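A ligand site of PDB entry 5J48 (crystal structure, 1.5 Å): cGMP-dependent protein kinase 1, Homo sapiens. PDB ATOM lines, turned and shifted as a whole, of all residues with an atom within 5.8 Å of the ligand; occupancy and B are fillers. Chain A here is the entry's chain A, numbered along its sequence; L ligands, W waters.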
ATOM      1  N   ILE A  48      -2.731   5.259  17.074  1.00  0.00           N
ATOM      2  CA  ILE A  48      -3.531   5.583  15.899  1.00  0.00           C
ATOM      3  C   ILE A  48      -4.797   4.744  15.979  1.00  0.00           C
ATOM      4  O   ILE A  48      -4.741   3.547  16.292  1.00  0.00           O
ATOM      5  CB  ILE A  48      -2.788   5.258  14.597  1.00  0.00           C
ATOM      6  CG1 ILE A  48      -1.634   6.228  14.365  1.00  0.00           C
ATOM      7  CG2 ILE A  48      -3.765   5.241  13.421  1.00  0.00           C
ATOM      8  CD1 ILE A  48      -0.805   5.897  13.134  1.00  0.00           C
ATOM      9  N   VAL A  67      -0.370  -3.703  15.307  1.00  0.00           N
ATOM     10  CA  VAL A  67      -1.146  -3.106  14.224  1.00  0.00           C
ATOM     11  C   VAL A  67      -2.322  -4.035  13.958  1.00  0.00           C
ATOM     12  O   VAL A  67      -2.127  -5.239  13.753  1.00  0.00           O
ATOM     13  CB  VAL A  67      -0.287  -2.948  12.951  1.00  0.00           C
ATOM     14  CG1 VAL A  67      -1.087  -2.184  11.895  1.00  0.00           C
ATOM     15  CG2 VAL A  67       0.992  -2.232  13.235  1.00  0.00           C
ATOM     16  N   ARG A  69      -6.668  -4.308  12.363  1.00  0.00           N
ATOM     17  CA  ARG A  69      -7.727  -3.751  11.522  1.00  0.00           C
ATOM     18  C   ARG A  69      -9.056  -4.360  11.916  1.00  0.00           C
ATOM     19  O   ARG A  69      -9.120  -5.529  12.304  1.00  0.00           O
ATOM     20  CB  ARG A  69      -7.474  -4.039  10.028  1.00  0.00           C
ATOM     21  CG  ARG A  69      -6.901  -2.871   9.297  1.00  0.00           C
ATOM     22  CD  ARG A  69      -6.488  -3.188   7.876  1.00  0.00           C
ATOM     23  NE  ARG A  69      -7.589  -3.495   6.989  1.00  0.00           N
ATOM     24  CZ  ARG A  69      -8.354  -2.594   6.364  1.00  0.00           C
ATOM     25  NH1 ARG A  69      -8.150  -1.282   6.502  1.00  0.00           N
ATOM     26  NH2 ARG A  69      -9.307  -3.021   5.560  1.00  0.00           N
ATOM     27  N   LEU A  80      -2.474  -7.707  12.404  1.00  0.00           N
ATOM     28  CA  LEU A  80      -1.664  -7.601  11.191  1.00  0.00           C
ATOM     29  C   LEU A  80      -0.193  -7.878  11.481  1.00  0.00           C
ATOM     30  O   LEU A  80       0.398  -8.783  10.869  1.00  0.00           O
ATOM     31  CB  LEU A  80      -1.854  -6.238  10.541  1.00  0.00           C
ATOM     32  CG  LEU A  80      -3.322  -5.889  10.244  1.00  0.00           C
ATOM     33  CD1 LEU A  80      -3.348  -4.539   9.561  1.00  0.00           C
ATOM     34  CD2 LEU A  80      -4.026  -6.931   9.420  1.00  0.00           C
ATOM     35  N   ARG A  81       0.402  -7.116  12.400  1.00  0.00           N
ATOM     36  CA  ARG A  81       1.817  -7.330  12.704  1.00  0.00           C
ATOM     37  C   ARG A  81       2.194  -6.554  13.948  1.00  0.00           C
ATOM     38  O   ARG A  81       1.427  -5.725  14.448  1.00  0.00           O
ATOM     39  CB  ARG A  81       2.720  -6.888  11.547  1.00  0.00           C
ATOM     40  CG  ARG A  81       2.844  -5.368  11.438  1.00  0.00           C
ATOM     41  CD  ARG A  81       3.539  -4.918  10.154  1.00  0.00           C
ATOM     42  NE  ARG A  81       2.636  -5.031   9.035  1.00  0.00           N
ATOM     43  CZ  ARG A  81       2.709  -5.942   8.081  1.00  0.00           C
ATOM     44  NH1 ARG A  81       3.679  -6.848   8.055  1.00  0.00           N
ATOM     45  NH2 ARG A  81       1.776  -5.940   7.132  1.00  0.00           N
ATOM     46  N   LEU A  83       5.480  -4.099  15.437  1.00  0.00           N
ATOM     47  CA  LEU A  83       6.638  -3.290  15.066  1.00  0.00           C
ATOM     48  C   LEU A  83       7.410  -2.956  16.319  1.00  0.00           C
ATOM     49  O   LEU A  83       6.872  -2.967  17.425  1.00  0.00           O
ATOM     50  CB  LEU A  83       6.244  -1.973  14.421  1.00  0.00           C
ATOM     51  CG  LEU A  83       5.366  -2.001  13.189  1.00  0.00           C
ATOM     52  CD1 LEU A  83       4.971  -0.562  12.859  1.00  0.00           C
ATOM     53  CD2 LEU A  83       6.076  -2.625  12.019  1.00  0.00           C
ATOM     54  N   TRP A  88       8.630   2.384  11.656  1.00  0.00           N
ATOM     55  CA  TRP A  88       7.838   3.592  11.534  1.00  0.00           C
ATOM     56  C   TRP A  88       6.467   3.242  10.993  1.00  0.00           C
ATOM     57  O   TRP A  88       6.234   2.141  10.463  1.00  0.00           O
ATOM     58  CB  TRP A  88       8.528   4.662  10.669  1.00  0.00           C
ATOM     59  CG  TRP A  88       9.083   4.167   9.396  1.00  0.00           C
ATOM     60  CD1 TRP A  88      10.386   3.821   9.164  1.00  0.00           C
ATOM     61  CD2 TRP A  88       8.391   3.944   8.168  1.00  0.00           C
ATOM     62  NE1 TRP A  88      10.534   3.393   7.883  1.00  0.00           N
ATOM     63  CE2 TRP A  88       9.331   3.472   7.231  1.00  0.00           C
ATOM     64  CE3 TRP A  88       7.065   4.106   7.758  1.00  0.00           C
ATOM     65  CZ2 TRP A  88       8.988   3.142   5.937  1.00  0.00           C
ATOM     66  CZ3 TRP A  88       6.730   3.789   6.471  1.00  0.00           C
ATOM     67  CH2 TRP A  88       7.696   3.313   5.565  1.00  0.00           C
ATOM     68  N   PHE A  89       5.540   4.184  11.132  1.00  0.00           N
ATOM     69  CA  PHE A  89       4.167   3.931  10.708  1.00  0.00           C
ATOM     70  C   PHE A  89       3.410   5.248  10.636  1.00  0.00           C
ATOM     71  O   PHE A  89       3.843   6.273  11.162  1.00  0.00           O
ATOM     72  CB  PHE A  89       3.453   2.948  11.643  1.00  0.00           C
ATOM     73  CG  PHE A  89       3.385   3.406  13.083  1.00  0.00           C
ATOM     74  CD1 PHE A  89       2.336   4.208  13.526  1.00  0.00           C
ATOM     75  CD2 PHE A  89       4.364   3.043  14.002  1.00  0.00           C
ATOM     76  CE1 PHE A  89       2.264   4.677  14.815  1.00  0.00           C
ATOM     77  CE2 PHE A  89       4.284   3.484  15.307  1.00  0.00           C
ATOM     78  CZ  PHE A  89       3.235   4.301  15.726  1.00  0.00           C
ATOM     79  N   GLY A  90       2.271   5.206   9.968  1.00  0.00           N
ATOM     80  CA  GLY A  90       1.380   6.339   9.892  1.00  0.00           C
ATOM     81  C   GLY A  90       1.504   7.147   8.629  1.00  0.00           C
ATOM     82  O   GLY A  90       1.000   8.281   8.585  1.00  0.00           O
ATOM     83  N   GLU A  91       2.178   6.618   7.591  1.00  0.00           N
ATOM     84  CA  GLU A  91       2.384   7.337   6.339  1.00  0.00           C
ATOM     85  C   GLU A  91       1.181   7.272   5.409  1.00  0.00           C
ATOM     86  O   GLU A  91       1.038   8.156   4.557  1.00  0.00           O
ATOM     87  CB  GLU A  91       3.647   6.812   5.651  1.00  0.00           C
ATOM     88  CG  GLU A  91       3.486   5.647   4.650  1.00  0.00           C
ATOM     89  CD  GLU A  91       3.139   4.296   5.276  1.00  0.00           C
ATOM     90  OE1 GLU A  91       3.020   4.159   6.501  1.00  0.00           O
ATOM     91  OE2 GLU A  91       3.008   3.345   4.472  1.00  0.00           O
ATOM     92  N   LYS A  92       0.316   6.261   5.515  1.00  0.00           N
ATOM     93  CA  LYS A  92      -0.713   6.105   4.494  1.00  0.00           C
ATOM     94  C   LYS A  92      -1.670   7.289   4.466  1.00  0.00           C
ATOM     95  O   LYS A  92      -2.079   7.733   3.388  1.00  0.00           O
ATOM     96  CB  LYS A  92      -1.469   4.793   4.681  1.00  0.00           C
ATOM     97  CG  LYS A  92      -0.601   3.595   4.495  1.00  0.00           C
ATOM     98  CD  LYS A  92      -1.386   2.315   4.709  1.00  0.00           C
ATOM     99  CE  LYS A  92      -2.370   2.105   3.606  1.00  0.00           C
ATOM    100  NZ  LYS A  92      -3.121   0.820   3.818  1.00  0.00           N
ATOM    101  N   ALA A  93      -2.042   7.805   5.644  1.00  0.00           N
ATOM    102  CA  ALA A  93      -2.942   8.951   5.734  1.00  0.00           C
ATOM    103  C   ALA A  93      -2.302  10.255   5.277  1.00  0.00           C
ATOM    104  O   ALA A  93      -3.020  11.240   5.118  1.00  0.00           O
ATOM    105  CB  ALA A  93      -3.450   9.109   7.174  1.00  0.00           C
ATOM    106  N   LEU A  94      -0.994  10.279   5.023  1.00  0.00           N
ATOM    107  CA  LEU A  94      -0.318  11.499   4.630  1.00  0.00           C
ATOM    108  C   LEU A  94      -0.188  11.633   3.121  1.00  0.00           C
ATOM    109  O   LEU A  94       0.401  12.622   2.655  1.00  0.00           O
ATOM    110  CB  LEU A  94       1.048  11.540   5.306  1.00  0.00           C
ATOM    111  CG  LEU A  94       1.006  11.316   6.810  1.00  0.00           C
ATOM    112  CD1 LEU A  94       2.396  11.449   7.425  1.00  0.00           C
ATOM    113  CD2 LEU A  94       0.052  12.258   7.504  1.00  0.00           C
ATOM    114  N   VAL A  99      -7.382   9.206   5.804  1.00  0.00           N
ATOM    115  CA  VAL A  99      -8.006   8.346   6.797  1.00  0.00           C
ATOM    116  C   VAL A  99      -7.010   7.299   7.239  1.00  0.00           C
ATOM    117  O   VAL A  99      -6.286   6.703   6.426  1.00  0.00           O
ATOM    118  CB  VAL A  99      -9.257   7.675   6.208  1.00  0.00           C
ATOM    119  CG1 VAL A  99      -8.893   6.811   5.033  1.00  0.00           C
ATOM    120  CG2 VAL A  99      -9.962   6.875   7.262  1.00  0.00           C
ATOM    121  N   ARG A 100      -6.952   7.074   8.543  1.00  0.00           N
ATOM    122  CA  ARG A 100      -6.142   6.011   9.110  1.00  0.00           C
ATOM    123  C   ARG A 100      -6.769   4.672   8.758  1.00  0.00           C
ATOM    124  O   ARG A 100      -7.971   4.465   8.942  1.00  0.00           O
ATOM    125  CB  ARG A 100      -6.086   6.139  10.629  1.00  0.00           C
ATOM    126  CG  ARG A 100      -5.393   7.403  11.125  1.00  0.00           C
ATOM    127  CD  ARG A 100      -3.960   7.450  10.719  1.00  0.00           C
ATOM    128  NE  ARG A 100      -3.239   8.405  11.532  1.00  0.00           N
ATOM    129  CZ  ARG A 100      -2.000   8.823  11.254  1.00  0.00           C
ATOM    130  NH1 ARG A 100      -1.357   8.385  10.189  1.00  0.00           N
ATOM    131  NH2 ARG A 100      -1.433   9.719  12.056  1.00  0.00           N
ATOM    132  N   THR A 101      -5.926   3.762   8.250  1.00  0.00           N
ATOM    133  CA  THR A 101      -6.380   2.491   7.698  1.00  0.00           C
ATOM    134  C   THR A 101      -6.168   1.312   8.627  1.00  0.00           C
ATOM    135  O   THR A 101      -6.517   0.201   8.256  1.00  0.00           O
ATOM    136  CB  THR A 101      -5.669   2.198   6.374  1.00  0.00           C
ATOM    137  OG1 THR A 101      -4.277   1.946   6.589  1.00  0.00           O
ATOM    138  CG2 THR A 101      -5.875   3.335   5.370  1.00  0.00           C
ATOM    139  N   ALA A 102      -5.625   1.533   9.821  1.00  0.00           N
ATOM    140  CA  ALA A 102      -5.397   0.487  10.805  1.00  0.00           C
ATOM    141  C   ALA A 102      -5.211   1.172  12.142  1.00  0.00           C
ATOM    142  O   ALA A 102      -4.958   2.365  12.199  1.00  0.00           O
ATOM    143  CB  ALA A 102      -4.152  -0.363  10.481  1.00  0.00           C
ATOM    144  N   ASN A 103      -5.375   0.395  13.209  1.00  0.00           N
ATOM    145  CA  ASN A 103      -5.023   0.823  14.547  1.00  0.00           C
ATOM    146  C   ASN A 103      -3.561   0.490  14.811  1.00  0.00           C
ATOM    147  O   ASN A 103      -3.054  -0.521  14.333  1.00  0.00           O
ATOM    148  CB  ASN A 103      -5.824   0.020  15.575  1.00  0.00           C
ATOM    149  CG  ASN A 103      -7.301   0.105  15.358  1.00  0.00           C
ATOM    150  OD1 ASN A 103      -7.901   1.185  15.439  1.00  0.00           O
ATOM    151  ND2 ASN A 103      -7.933  -1.030  15.139  1.00  0.00           N
ATOM    152  N   VAL A 104      -2.913   1.333  15.606  1.00  0.00           N
ATOM    153  CA  VAL A 104      -1.573   1.053  16.094  1.00  0.00           C
ATOM    154  C   VAL A 104      -1.620   1.258  17.602  1.00  0.00           C
ATOM    155  O   VAL A 104      -1.984   2.350  18.063  1.00  0.00           O
ATOM    156  CB  VAL A 104      -0.495   1.920  15.443  1.00  0.00           C
ATOM    157  CG1 VAL A 104       0.884   1.487  15.920  1.00  0.00           C
ATOM    158  CG2 VAL A 104      -0.551   1.772  13.936  1.00  0.00           C
ATOM    159  N   ASP A 129      11.521   4.915  -0.171  1.00  0.00           N
ATOM    160  CA  ASP A 129      11.488   3.956   0.934  1.00  0.00           C
ATOM    161  C   ASP A 129      10.207   4.117   1.748  1.00  0.00           C
ATOM    162  O   ASP A 129       9.617   3.128   2.190  1.00  0.00           O
ATOM    163  CB  ASP A 129      12.710   4.148   1.826  1.00  0.00           C
ATOM    164  N   LYS A 133       6.797   1.967  -0.681  1.00  0.00           N
ATOM    165  CA  LYS A 133       7.083   0.665  -0.102  1.00  0.00           C
ATOM    166  C   LYS A 133       5.879  -0.241  -0.303  1.00  0.00           C
ATOM    167  O   LYS A 133       4.730   0.212  -0.354  1.00  0.00           O
ATOM    168  CB  LYS A 133       7.352   0.786   1.397  1.00  0.00           C
ATOM    169  N   ALA A 134       6.139  -1.541  -0.418  1.00  0.00           N
ATOM    170  CA  ALA A 134       5.094  -2.530  -0.630  1.00  0.00           C
ATOM    171  C   ALA A 134       4.962  -3.393   0.608  1.00  0.00           C
ATOM    172  O   ALA A 134       5.953  -3.949   1.102  1.00  0.00           O
ATOM    173  CB  ALA A 134       5.427  -3.390  -1.844  1.00  0.00           C
ATOM    174  N   TYR A 135       3.740  -3.498   1.120  1.00  0.00           N
ATOM    175  CA  TYR A 135       3.447  -4.367   2.255  1.00  0.00           C
ATOM    176  C   TYR A 135       1.943  -4.571   2.376  1.00  0.00           C
ATOM    177  O   TYR A 135       1.189  -4.194   1.481  1.00  0.00           O
ATOM    178  CB  TYR A 135       4.016  -3.773   3.552  1.00  0.00           C
ATOM    179  CG  TYR A 135       3.415  -2.443   3.952  1.00  0.00           C
ATOM    180  CD1 TYR A 135       3.947  -1.254   3.492  1.00  0.00           C
ATOM    181  CD2 TYR A 135       2.323  -2.385   4.819  1.00  0.00           C
ATOM    182  CE1 TYR A 135       3.407  -0.030   3.868  1.00  0.00           C
ATOM    183  CE2 TYR A 135       1.770  -1.168   5.191  1.00  0.00           C
ATOM    184  CZ  TYR A 135       2.323  -0.002   4.725  1.00  0.00           C
ATOM    185  OH  TYR A 135       1.780   1.207   5.100  1.00  0.00           O
HETATM  186  C1  LIG L   1      -1.033  -3.213   7.298  1.00  0.00           C
HETATM  187  N1  LIG L   1      -2.195  -2.643   6.829  1.00  0.00           N
HETATM  188  C2  LIG L   1      -2.487  -1.284   7.031  1.00  0.00           C
HETATM  189  C3  LIG L   1       1.444  -1.396   9.154  1.00  0.00           C
HETATM  190  C4  LIG L   1       4.506   0.384   8.376  1.00  0.00           C
HETATM  191  C5  LIG L   1       5.392   0.577   7.331  1.00  0.00           C
HETATM  192  C6  LIG L   1       5.791  -0.500   6.557  1.00  0.00           C
HETATM  193  C7  LIG L   1       4.442  -1.959   7.890  1.00  0.00           C
HETATM  194 CL1  LIG L   1       6.919  -0.261   5.241  1.00  0.00          CL
HETATM  195  P1  LIG L   1      -2.029   4.812   8.399  1.00  0.00           P
HETATM  196  C8  LIG L   1      -2.104   3.049  10.454  1.00  0.00           C
HETATM  197  C9  LIG L   1      -0.788   2.498  10.031  1.00  0.00           C
HETATM  198  C10 LIG L   1      -0.513   2.703   8.332  1.00  0.00           C
HETATM  199  C11 LIG L   1       0.568   1.985   8.148  1.00  0.00           C
HETATM  200  C12 LIG L   1       0.656   0.790   9.306  1.00  0.00           C
HETATM  201  O1  LIG L   1      -0.511   1.254  10.272  1.00  0.00           O
HETATM  202  N2  LIG L   1       0.545  -0.408   8.923  1.00  0.00           N
HETATM  203  C13 LIG L   1      -0.423  -0.992   8.230  1.00  0.00           C
HETATM  204  C14 LIG L   1      -0.126  -2.316   8.042  1.00  0.00           C
HETATM  205  O2  LIG L   1      -0.794  -4.402   7.110  1.00  0.00           O
HETATM  206  N3  LIG L   1      -1.628  -0.416   7.732  1.00  0.00           N
HETATM  207  N4  LIG L   1      -3.663  -0.769   6.553  1.00  0.00           N
HETATM  208  N5  LIG L   1       1.079  -2.588   8.643  1.00  0.00           N
HETATM  209  S1  LIG L   1       2.935  -1.160   9.998  1.00  0.00           S
HETATM  210  C15 LIG L   1       4.041  -0.889   8.652  1.00  0.00           C
HETATM  211  C16 LIG L   1       5.323  -1.772   6.850  1.00  0.00           C
HETATM  212  O3  LIG L   1       1.747   2.822   8.373  1.00  0.00           O
HETATM  213  O4  LIG L   1      -0.632   4.088   7.952  1.00  0.00           O
HETATM  214  O5  LIG L   1      -1.874   6.278   8.258  1.00  0.00           O
HETATM  215  O6  LIG L   1      -2.170   4.513  10.039  1.00  0.00           O
HETATM  216  O7  LIG L   1      -3.235   4.181   7.661  1.00  0.00           O
HETATM  217  O   HOH W   1      -1.352  -1.172   3.806  1.00  0.00           O
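The side-chain hydroxyl (OH) of Tyr 135 sits at hydrogen-bond distance from the side-chain carboxylate (OE2) of Glu 91, at 2.5 Å.
O of Ile 48 is in hydrogen-bond range of N of Val 104, 3.0 Å away.
The side-chain hydroxyl of Thr 101 is in hydrogen-bond range of the side-chain amino group of Lys 92 (3.2 Å).
O of Gly 90 sits at hydrogen-bond distance from NH1 of Arg 100, at 2.9 Å.
The backbone carbonyl oxygen (O) of Thr 101 sits at hydrogen-bond distance from the guanidinium group (NH1) of Arg 69 (2.8 Å).
The backbone carbonyl oxygen (O) of Arg 81 is in hydrogen-bond range of the backbone NH (N) of Val 67, 2.8 Å away.
N of Leu 80 is in hydrogen-bond range of O of Val 67.
Water W1 bridges NZ of Lys 92 and N1 of the ligand.
Residues that only touch the ligand: Trp 88, Tyr 135, Ala 102, Leu 80, Phe 89, Leu 83, Ile 48, Val 104, Val 67 and Arg 69.
Hydrophobic or aromatic side chains within 4 Å of the ligand: Ile 48, Val 67, Leu 80, Leu 83, Trp 88, Phe 89, Ala 93, Ala 102, Val 104 and Tyr 135.
17 residues have an atom within 4 Å of the ligand: Ile 48, Val 67, Arg 69, Leu 80, Arg 81, Leu 83, Trp 88, Phe 89, Gly 90, Glu 91, Lys 92, Ala 93, Arg 100, Thr 101, Ala 102, Val 104 and Tyr 135.
The backbone NH (N) of Ala 93 is in hydrogen-bond range of an oxygen (O5) of the ligand, 3.0 Å away.
N of Thr 101 lies within hydrogen-bond range of O7 of the ligand, at 2.8 Å.
NH1 of Arg 100 is in salt-bridge range of O5 of the ligand (2.9 Å).
N of Lys 92 lies within hydrogen-bond range of O4 of the ligand (3.4 Å).
N of Gly 90 is in hydrogen-bond range of O3 of the ligand, 2.9 Å away.
An oxygen (O7) of the ligand lies within hydrogen-bond range of the side-chain hydroxyl of Thr 101 (2.7 Å).
OE1 of Glu 91 lies within hydrogen-bond range of O3 of the ligand (2.6 Å).
The guanidinium group (NE) of Arg 81 lies within hydrogen-bond range of a nitrogen (N5) of the ligand, at 2.9 Å.
The backbone carbonyl oxygen (O) of Thr 101 is in hydrogen-bond range of a nitrogen (N4) of the ligand.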
